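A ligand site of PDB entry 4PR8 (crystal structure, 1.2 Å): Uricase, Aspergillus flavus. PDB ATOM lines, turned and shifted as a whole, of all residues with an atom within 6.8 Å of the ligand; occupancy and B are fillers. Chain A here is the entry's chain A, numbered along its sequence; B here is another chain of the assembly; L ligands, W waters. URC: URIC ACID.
An oxygen (O24) of the ligand lies within hydrogen-bond range of the backbone NH (N) of Thr 58 of chain B (3.2 Å). The side-chain hydroxyl of Thr 58 of chain B lies within hydrogen-bond range of an oxygen (O24) of the ligand (3.2 Å). N of Asp 59 of chain B is in hydrogen-bond range of O24 of the ligand (2.8 Å). N of Val 228 is in hydrogen-bond range of O11 of the ligand, 2.9 Å away. The guanidinium group (NH2) of Arg 177 is in hydrogen-bond range of an oxygen (O11) of the ligand. NE2 of Gln 229 sits at hydrogen-bond distance from O13 of the ligand, 2.9 Å away. The side-chain amide nitrogen (ND2) of Asn 255 sits close to a nitrogen (N3) of the ligand (3.5 Å).
The side-chain amino group (NZ) of Lys 11 of chain B sits at hydrogen-bond distance from the side-chain hydroxyl (OG1) of Thr 58 of chain B, at 3.0 Å. The backbone NH of Arg 177 lies within hydrogen-bond range of the backbone carbonyl oxygen of Ser 158 (2.9 Å). The backbone carbonyl oxygen (O) of Ser 227 is in hydrogen-bond range of the side-chain hydroxyl (OG) of Ser 225. The backbone NH (N) of Asn 255 is in hydrogen-bond range of the backbone carbonyl oxygen (O) of Gly 287 (2.8 Å). OH of Tyr 9 of chain B sits at hydrogen-bond distance from O of Val 56 of chain B (2.6 Å).
Residues that only touch the ligand: Phe 160 (3.3 Å), Ser 227 (3.4 Å), Leu 171 (3.5 Å), Ile 55 of chain B (3.5 Å), Ala 57 of chain B (3.6 Å) and Tyr 9 of chain B (3.7 Å). Hydrophobic or aromatic side chains that line the ligand: Phe 160, Leu 171, Val 228, Tyr 9 of chain B, Ile 55 of chain B and Ala 57 of chain B. 12 residues have an atom within 4 Å of the ligand: Phe 160, Leu 171, Arg 177, Ser 227, Val 228, Gln 229, Asn 255, Tyr 9 of chain B, Ile 55 of chain B, Ala 57 of chain B, Thr 58 of chain B and Asp 59 of chain B. The nearest printed residue that does not touch the ligand is Ile 289 (4.1 Å).
Water W1 bridges N9 of the ligand (3.0 Å) and NH1 of Arg 177 (3.3 Å).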
ATOM      1  N   SER A 158      26.426  11.930 -21.071  1.00  0.00           N
ATOM      2  CA  SER A 158      26.208  10.735 -21.843  1.00  0.00           C
ATOM      3  C   SER A 158      26.608  11.027 -23.285  1.00  0.00           C
ATOM      4  O   SER A 158      26.270  12.099 -23.808  1.00  0.00           O
ATOM      5  CB  SER A 158      24.752  10.252 -21.765  1.00  0.00           C
ATOM      6  OG  SER A 158      24.502   9.159 -22.623  1.00  0.00           O
ATOM      7  N   GLN A 159      27.310  10.097 -23.907  1.00  0.00           N
ATOM      8  CA  GLN A 159      27.772  10.232 -25.281  1.00  0.00           C
ATOM      9  C   GLN A 159      27.459   8.962 -26.040  1.00  0.00           C
ATOM     10  O   GLN A 159      27.224   7.901 -25.442  1.00  0.00           O
ATOM     11  CB  GLN A 159      29.279  10.508 -25.279  1.00  0.00           C
ATOM     12  CG  GLN A 159      29.705  11.663 -24.392  1.00  0.00           C
ATOM     13  CD  GLN A 159      31.189  11.983 -24.592  1.00  0.00           C
ATOM     14  OE1 GLN A 159      31.714  11.995 -25.700  1.00  0.00           O
ATOM     15  NE2 GLN A 159      31.912  12.232 -23.529  1.00  0.00           N
ATOM     16  N   PHE A 160      27.472   9.036 -27.368  1.00  0.00           N
ATOM     17  CA  PHE A 160      27.387   7.859 -28.194  1.00  0.00           C
ATOM     18  C   PHE A 160      27.907   8.201 -29.596  1.00  0.00           C
ATOM     19  O   PHE A 160      27.201   8.796 -30.413  1.00  0.00           O
ATOM     20  CB  PHE A 160      25.961   7.294 -28.221  1.00  0.00           C
ATOM     21  CG  PHE A 160      25.906   5.902 -28.837  1.00  0.00           C
ATOM     22  CD1 PHE A 160      26.639   4.878 -28.200  1.00  0.00           C
ATOM     23  CD2 PHE A 160      25.207   5.570 -29.941  1.00  0.00           C
ATOM     24  CE1 PHE A 160      26.599   3.630 -28.764  1.00  0.00           C
ATOM     25  CE2 PHE A 160      25.190   4.317 -30.520  1.00  0.00           C
ATOM     26  CZ  PHE A 160      25.926   3.299 -29.905  1.00  0.00           C
ATOM     27  N   PHE A 163      30.168   4.332 -33.324  1.00  0.00           N
ATOM     28  CA  PHE A 163      29.500   3.092 -33.643  1.00  0.00           C
ATOM     29  C   PHE A 163      29.573   2.764 -35.125  1.00  0.00           C
ATOM     30  O   PHE A 163      29.914   3.634 -35.938  1.00  0.00           O
ATOM     31  CB  PHE A 163      28.025   3.104 -33.185  1.00  0.00           C
ATOM     32  CG  PHE A 163      27.291   4.385 -33.593  1.00  0.00           C
ATOM     33  CD1 PHE A 163      27.313   5.493 -32.784  1.00  0.00           C
ATOM     34  CD2 PHE A 163      26.624   4.379 -34.781  1.00  0.00           C
ATOM     35  CE1 PHE A 163      26.612   6.630 -33.214  1.00  0.00           C
ATOM     36  CE2 PHE A 163      25.904   5.486 -35.217  1.00  0.00           C
ATOM     37  CZ  PHE A 163      25.928   6.581 -34.402  1.00  0.00           C
ATOM     38  N   LEU A 171      21.631   7.381 -37.697  1.00  0.00           N
ATOM     39  CA  LEU A 171      21.840   8.077 -36.443  1.00  0.00           C
ATOM     40  C   LEU A 171      23.084   8.930 -36.453  1.00  0.00           C
ATOM     41  O   LEU A 171      24.186   8.465 -36.771  1.00  0.00           O
ATOM     42  CB  LEU A 171      21.947   7.047 -35.300  1.00  0.00           C
ATOM     43  CG  LEU A 171      22.180   7.528 -33.892  1.00  0.00           C
ATOM     44  CD1 LEU A 171      20.941   8.221 -33.341  1.00  0.00           C
ATOM     45  CD2 LEU A 171      22.581   6.361 -33.001  1.00  0.00           C
ATOM     46  N   ARG A 177      24.215  13.915 -24.799  1.00  0.00           N
ATOM     47  CA  ARG A 177      22.810  13.530 -24.936  1.00  0.00           C
ATOM     48  C   ARG A 177      22.251  13.261 -23.535  1.00  0.00           C
ATOM     49  O   ARG A 177      22.977  13.198 -22.561  1.00  0.00           O
ATOM     50  CB  ARG A 177      22.594  12.306 -25.794  1.00  0.00           C
ATOM     51  CG  ARG A 177      23.269  11.071 -25.202  1.00  0.00           C
ATOM     52  CD  ARG A 177      23.073   9.824 -26.063  1.00  0.00           C
ATOM     53  NE  ARG A 177      23.522   8.637 -25.319  1.00  0.00           N
ATOM     54  CZ  ARG A 177      23.337   7.424 -25.811  1.00  0.00           C
ATOM     55  NH1 ARG A 177      22.768   7.107 -26.947  1.00  0.00           N
ATOM     56  NH2 ARG A 177      23.770   6.411 -25.053  1.00  0.00           N
ATOM     57  N   LEU A 179      20.516  10.628 -21.007  1.00  0.00           N
ATOM     58  CA  LEU A 179      20.346   9.185 -20.818  1.00  0.00           C
ATOM     59  C   LEU A 179      19.350   8.914 -19.675  1.00  0.00           C
ATOM     60  O   LEU A 179      19.543   9.426 -18.597  1.00  0.00           O
ATOM     61  CB  LEU A 179      21.687   8.525 -20.511  1.00  0.00           C
ATOM     62  CG  LEU A 179      21.662   7.031 -20.146  1.00  0.00           C
ATOM     63  CD1 LEU A 179      21.122   6.211 -21.294  1.00  0.00           C
ATOM     64  CD2 LEU A 179      23.062   6.575 -19.730  1.00  0.00           C
ATOM     65  N   SER A 225      29.347   8.723 -19.787  1.00  0.00           N
ATOM     66  CA  SER A 225      29.058   7.441 -20.377  1.00  0.00           C
ATOM     67  C   SER A 225      29.363   7.393 -21.864  1.00  0.00           C
ATOM     68  O   SER A 225      28.869   8.166 -22.674  1.00  0.00           O
ATOM     69  CB  SER A 225      27.591   7.064 -20.139  1.00  0.00           C
ATOM     70  OG  SER A 225      27.129   6.076 -20.988  1.00  0.00           O
ATOM     71  N   ALA A 226      30.171   6.408 -22.242  1.00  0.00           N
ATOM     72  CA  ALA A 226      30.501   6.153 -23.625  1.00  0.00           C
ATOM     73  C   ALA A 226      29.406   5.430 -24.370  1.00  0.00           C
ATOM     74  O   ALA A 226      29.291   5.441 -25.574  1.00  0.00           O
ATOM     75  CB  ALA A 226      31.804   5.321 -23.660  1.00  0.00           C
ATOM     76  N   SER A 227      28.576   4.714 -23.577  1.00  0.00           N
ATOM     77  CA  SER A 227      27.440   3.961 -24.042  1.00  0.00           C
ATOM     78  C   SER A 227      26.766   3.294 -22.807  1.00  0.00           C
ATOM     79  O   SER A 227      27.358   3.289 -21.754  1.00  0.00           O
ATOM     80  CB  SER A 227      27.716   2.881 -25.070  1.00  0.00           C
ATOM     81  OG  SER A 227      28.591   1.917 -24.537  1.00  0.00           O
ATOM     82  N   VAL A 228      25.568   2.801 -23.066  1.00  0.00           N
ATOM     83  CA  VAL A 228      24.878   2.068 -21.981  1.00  0.00           C
ATOM     84  C   VAL A 228      25.689   0.825 -21.636  1.00  0.00           C
ATOM     85  O   VAL A 228      25.882   0.520 -20.449  1.00  0.00           O
ATOM     86  CB  VAL A 228      23.451   1.727 -22.413  1.00  0.00           C
ATOM     87  CG1 VAL A 228      22.759   0.836 -21.382  1.00  0.00           C
ATOM     88  CG2 VAL A 228      22.616   2.997 -22.591  1.00  0.00           C
ATOM     89  N   GLN A 229      26.153   0.147 -22.668  1.00  0.00           N
ATOM     90  CA  GLN A 229      27.012  -1.034 -22.482  1.00  0.00           C
ATOM     91  C   GLN A 229      28.128  -0.840 -21.486  1.00  0.00           C
ATOM     92  O   GLN A 229      28.370  -1.601 -20.539  1.00  0.00           O
ATOM     93  CB  GLN A 229      27.535  -1.384 -23.878  1.00  0.00           C
ATOM     94  CG  GLN A 229      26.584  -1.987 -24.861  1.00  0.00           C
ATOM     95  CD  GLN A 229      25.774  -1.021 -25.719  1.00  0.00           C
ATOM     96  OE1 GLN A 229      25.604   0.133 -25.296  1.00  0.00           O
ATOM     97  NE2 GLN A 229      25.311  -1.515 -26.843  1.00  0.00           N
ATOM     98  N   ASN A 255      17.144   1.980 -23.164  1.00  0.00           N
ATOM     99  CA  ASN A 255      17.524   3.390 -23.409  1.00  0.00           C
ATOM    100  C   ASN A 255      16.260   4.135 -23.842  1.00  0.00           C
ATOM    101  O   ASN A 255      15.776   3.917 -24.926  1.00  0.00           O
ATOM    102  CB  ASN A 255      18.607   3.404 -24.469  1.00  0.00           C
ATOM    103  CG  ASN A 255      19.290   4.746 -24.560  1.00  0.00           C
ATOM    104  OD1 ASN A 255      18.920   5.753 -23.967  1.00  0.00           O
ATOM    105  ND2 ASN A 255      20.396   4.758 -25.310  1.00  0.00           N
ATOM    106  N   HIS A 257      14.604   6.978 -25.029  1.00  0.00           N
ATOM    107  CA  HIS A 257      15.119   8.099 -25.807  1.00  0.00           C
ATOM    108  C   HIS A 257      14.361   9.419 -25.579  1.00  0.00           C
ATOM    109  O   HIS A 257      13.145   9.415 -25.515  1.00  0.00           O
ATOM    110  CB  HIS A 257      15.105   7.731 -27.289  1.00  0.00           C
ATOM    111  CG  HIS A 257      15.761   6.430 -27.663  1.00  0.00           C
ATOM    112  ND1 HIS A 257      17.101   6.214 -27.434  1.00  0.00           N
ATOM    113  CD2 HIS A 257      15.265   5.339 -28.249  1.00  0.00           C
ATOM    114  CE1 HIS A 257      17.353   4.959 -27.875  1.00  0.00           C
ATOM    115  NE2 HIS A 257      16.280   4.406 -28.382  1.00  0.00           N
ATOM    116  N   GLY A 287      15.943   1.438 -27.055  1.00  0.00           N
ATOM    117  CA  GLY A 287      17.061   0.468 -27.000  1.00  0.00           C
ATOM    118  C   GLY A 287      16.855  -0.459 -25.817  1.00  0.00           C
ATOM    119  O   GLY A 287      16.275  -0.062 -24.805  1.00  0.00           O
ATOM    120  N   ILE A 289      19.449  -3.074 -23.681  1.00  0.00           N
ATOM    121  CA  ILE A 289      20.861  -3.446 -23.527  1.00  0.00           C
ATOM    122  C   ILE A 289      20.992  -4.405 -22.348  1.00  0.00           C
ATOM    123  O   ILE A 289      20.552  -4.052 -21.265  1.00  0.00           O
ATOM    124  CB  ILE A 289      21.728  -2.213 -23.347  1.00  0.00           C
ATOM    125  CG1 ILE A 289      21.404  -1.026 -24.273  1.00  0.00           C
ATOM    126  CG2 ILE A 289      23.219  -2.575 -23.477  1.00  0.00           C
ATOM    127  CD1 ILE A 289      21.398  -1.361 -25.740  1.00  0.00           C
ATOM    128  N   TYR B   9      21.858  -7.143 -27.223  1.00  0.00           N
ATOM    129  CA  TYR B   9      21.458  -5.716 -27.203  1.00  0.00           C
ATOM    130  C   TYR B   9      20.694  -5.498 -28.503  1.00  0.00           C
ATOM    131  O   TYR B   9      20.874  -6.181 -29.508  1.00  0.00           O
ATOM    132  CB  TYR B   9      22.644  -4.740 -26.976  1.00  0.00           C
ATOM    133  CG  TYR B   9      23.220  -4.447 -28.335  1.00  0.00           C
ATOM    134  CD1 TYR B   9      23.964  -5.462 -28.950  1.00  0.00           C
ATOM    135  CD2 TYR B   9      22.994  -3.255 -29.007  1.00  0.00           C
ATOM    136  CE1 TYR B   9      24.504  -5.268 -30.209  1.00  0.00           C
ATOM    137  CE2 TYR B   9      23.512  -3.079 -30.279  1.00  0.00           C
ATOM    138  CZ  TYR B   9      24.263  -4.080 -30.851  1.00  0.00           C
ATOM    139  OH  TYR B   9      24.783  -3.917 -32.117  1.00  0.00           O
ATOM    140  N   GLY B  10      19.836  -4.474 -28.509  1.00  0.00           N
ATOM    141  CA  GLY B  10      19.100  -4.134 -29.708  1.00  0.00           C
ATOM    142  C   GLY B  10      17.940  -3.159 -29.433  1.00  0.00           C
ATOM    143  O   GLY B  10      18.033  -2.352 -28.527  1.00  0.00           O
ATOM    144  N   LYS B  11      16.928  -3.278 -30.273  1.00  0.00           N
ATOM    145  CA  LYS B  11      15.791  -2.342 -30.185  1.00  0.00           C
ATOM    146  C   LYS B  11      14.529  -3.154 -29.859  1.00  0.00           C
ATOM    147  O   LYS B  11      14.242  -4.141 -30.518  1.00  0.00           O
ATOM    148  CB  LYS B  11      15.613  -1.525 -31.449  1.00  0.00           C
ATOM    149  CG  LYS B  11      14.710  -0.292 -31.260  1.00  0.00           C
ATOM    150  CD  LYS B  11      15.447   0.804 -30.576  1.00  0.00           C
ATOM    151  CE  LYS B  11      15.807   2.006 -31.408  1.00  0.00           C
ATOM    152  NZ  LYS B  11      16.754   2.879 -30.665  1.00  0.00           N
ATOM    153  N   ASN B  52      32.906   1.230 -29.298  1.00  0.00           N
ATOM    154  CA  ASN B  52      31.626   1.203 -29.996  1.00  0.00           C
ATOM    155  C   ASN B  52      31.677   0.767 -31.429  1.00  0.00           C
ATOM    156  O   ASN B  52      30.671   0.568 -32.116  1.00  0.00           O
ATOM    157  CB  ASN B  52      30.999   2.620 -29.919  1.00  0.00           C
ATOM    158  CG  ASN B  52      30.483   2.910 -28.533  1.00  0.00           C
ATOM    159  OD1 ASN B  52      30.230   1.974 -27.751  1.00  0.00           O
ATOM    160  ND2 ASN B  52      30.288   4.177 -28.224  1.00  0.00           N
ATOM    161  N   ILE B  55      29.469  -2.005 -32.301  1.00  0.00           N
ATOM    162  CA  ILE B  55      28.026  -1.830 -32.174  1.00  0.00           C
ATOM    163  C   ILE B  55      27.324  -1.461 -33.468  1.00  0.00           C
ATOM    164  O   ILE B  55      27.619  -0.366 -34.007  1.00  0.00           O
ATOM    165  CB  ILE B  55      27.723  -0.779 -31.088  1.00  0.00           C
ATOM    166  CG1 ILE B  55      28.332  -1.117 -29.735  1.00  0.00           C
ATOM    167  CG2 ILE B  55      26.212  -0.602 -30.934  1.00  0.00           C
ATOM    168  CD1 ILE B  55      28.164  -0.007 -28.703  1.00  0.00           C
ATOM    169  N   VAL B  56      26.456  -2.318 -33.962  1.00  0.00           N
ATOM    170  CA  VAL B  56      25.387  -2.016 -34.889  1.00  0.00           C
ATOM    171  C   VAL B  56      24.352  -1.223 -34.077  1.00  0.00           C
ATOM    172  O   VAL B  56      23.715  -1.799 -33.205  1.00  0.00           O
ATOM    173  CB  VAL B  56      24.739  -3.208 -35.571  1.00  0.00           C
ATOM    174  CG1 VAL B  56      23.555  -2.787 -36.434  1.00  0.00           C
ATOM    175  CG2 VAL B  56      25.771  -3.958 -36.424  1.00  0.00           C
ATOM    176  N   ALA B  57      24.260   0.082 -34.317  1.00  0.00           N
ATOM    177  CA  ALA B  57      23.416   0.922 -33.450  1.00  0.00           C
ATOM    178  C   ALA B  57      21.988   0.415 -33.425  1.00  0.00           C
ATOM    179  O   ALA B  57      21.421  -0.040 -34.410  1.00  0.00           O
ATOM    180  CB  ALA B  57      23.445   2.374 -33.895  1.00  0.00           C
ATOM    181  N   THR B  58      21.393   0.517 -32.215  1.00  0.00           N
ATOM    182  CA  THR B  58      20.028   0.008 -32.139  1.00  0.00           C
ATOM    183  C   THR B  58      19.100   0.817 -33.042  1.00  0.00           C
ATOM    184  O   THR B  58      18.118   0.292 -33.543  1.00  0.00           O
ATOM    185  CB  THR B  58      19.457  -0.016 -30.715  1.00  0.00           C
ATOM    186  OG1 THR B  58      19.232   1.327 -30.238  1.00  0.00           O
ATOM    187  CG2 THR B  58      20.459  -0.617 -29.735  1.00  0.00           C
ATOM    188  N   ASP B  59      19.466   2.099 -33.233  1.00  0.00           N
ATOM    189  CA  ASP B  59      18.705   2.891 -34.195  1.00  0.00           C
ATOM    190  C   ASP B  59      18.771   2.315 -35.591  1.00  0.00           C
ATOM    191  O   ASP B  59      17.842   2.307 -36.385  1.00  0.00           O
ATOM    192  CB  ASP B  59      19.222   4.333 -34.224  1.00  0.00           C
ATOM    193  CG  ASP B  59      18.351   5.218 -35.094  1.00  0.00           C
ATOM    194  OD1 ASP B  59      17.279   5.633 -34.589  1.00  0.00           O
ATOM    195  OD2 ASP B  59      18.701   5.499 -36.262  1.00  0.00           O
ATOM    196  N   SER B  60      19.978   1.786 -35.942  1.00  0.00           N
ATOM    197  CA  SER B  60      20.051   1.107 -37.215  1.00  0.00           C
ATOM    198  C   SER B  60      19.320  -0.216 -37.317  1.00  0.00           C
ATOM    199  O   SER B  60      18.785  -0.626 -38.332  1.00  0.00           O
ATOM    200  CB  SER B  60      21.550   0.857 -37.548  1.00  0.00           C
ATOM    201  OG  SER B  60      22.272   2.069 -37.391  1.00  0.00           O
HETATM  202  N1  URC L   1      24.085   2.044 -27.088  1.00  0.00           N
HETATM  203  C2  URC L   1      23.886   3.316 -26.615  1.00  0.00           C
HETATM  204  C6  URC L   1      23.650   1.515 -28.272  1.00  0.00           C
HETATM  205  N3  URC L   1      23.142   4.196 -27.384  1.00  0.00           N
HETATM  206  O11 URC L   1      24.379   3.586 -25.544  1.00  0.00           O
HETATM  207  C4  URC L   1      22.632   3.730 -28.531  1.00  0.00           C
HETATM  208  C5  URC L   1      22.864   2.451 -29.042  1.00  0.00           C
HETATM  209  N9  URC L   1      21.894   4.392 -29.484  1.00  0.00           N
HETATM  210  O13 URC L   1      23.838   0.361 -28.562  1.00  0.00           O
HETATM  211  N7  URC L   1      22.338   2.261 -30.228  1.00  0.00           N
HETATM  212  C8  URC L   1      21.740   3.427 -30.454  1.00  0.00           C
HETATM  213  O24 URC L   1      21.083   3.641 -31.472  1.00  0.00           O
HETATM  214  O   HOH W   1      20.412   7.008 -29.253  1.00  0.00           O
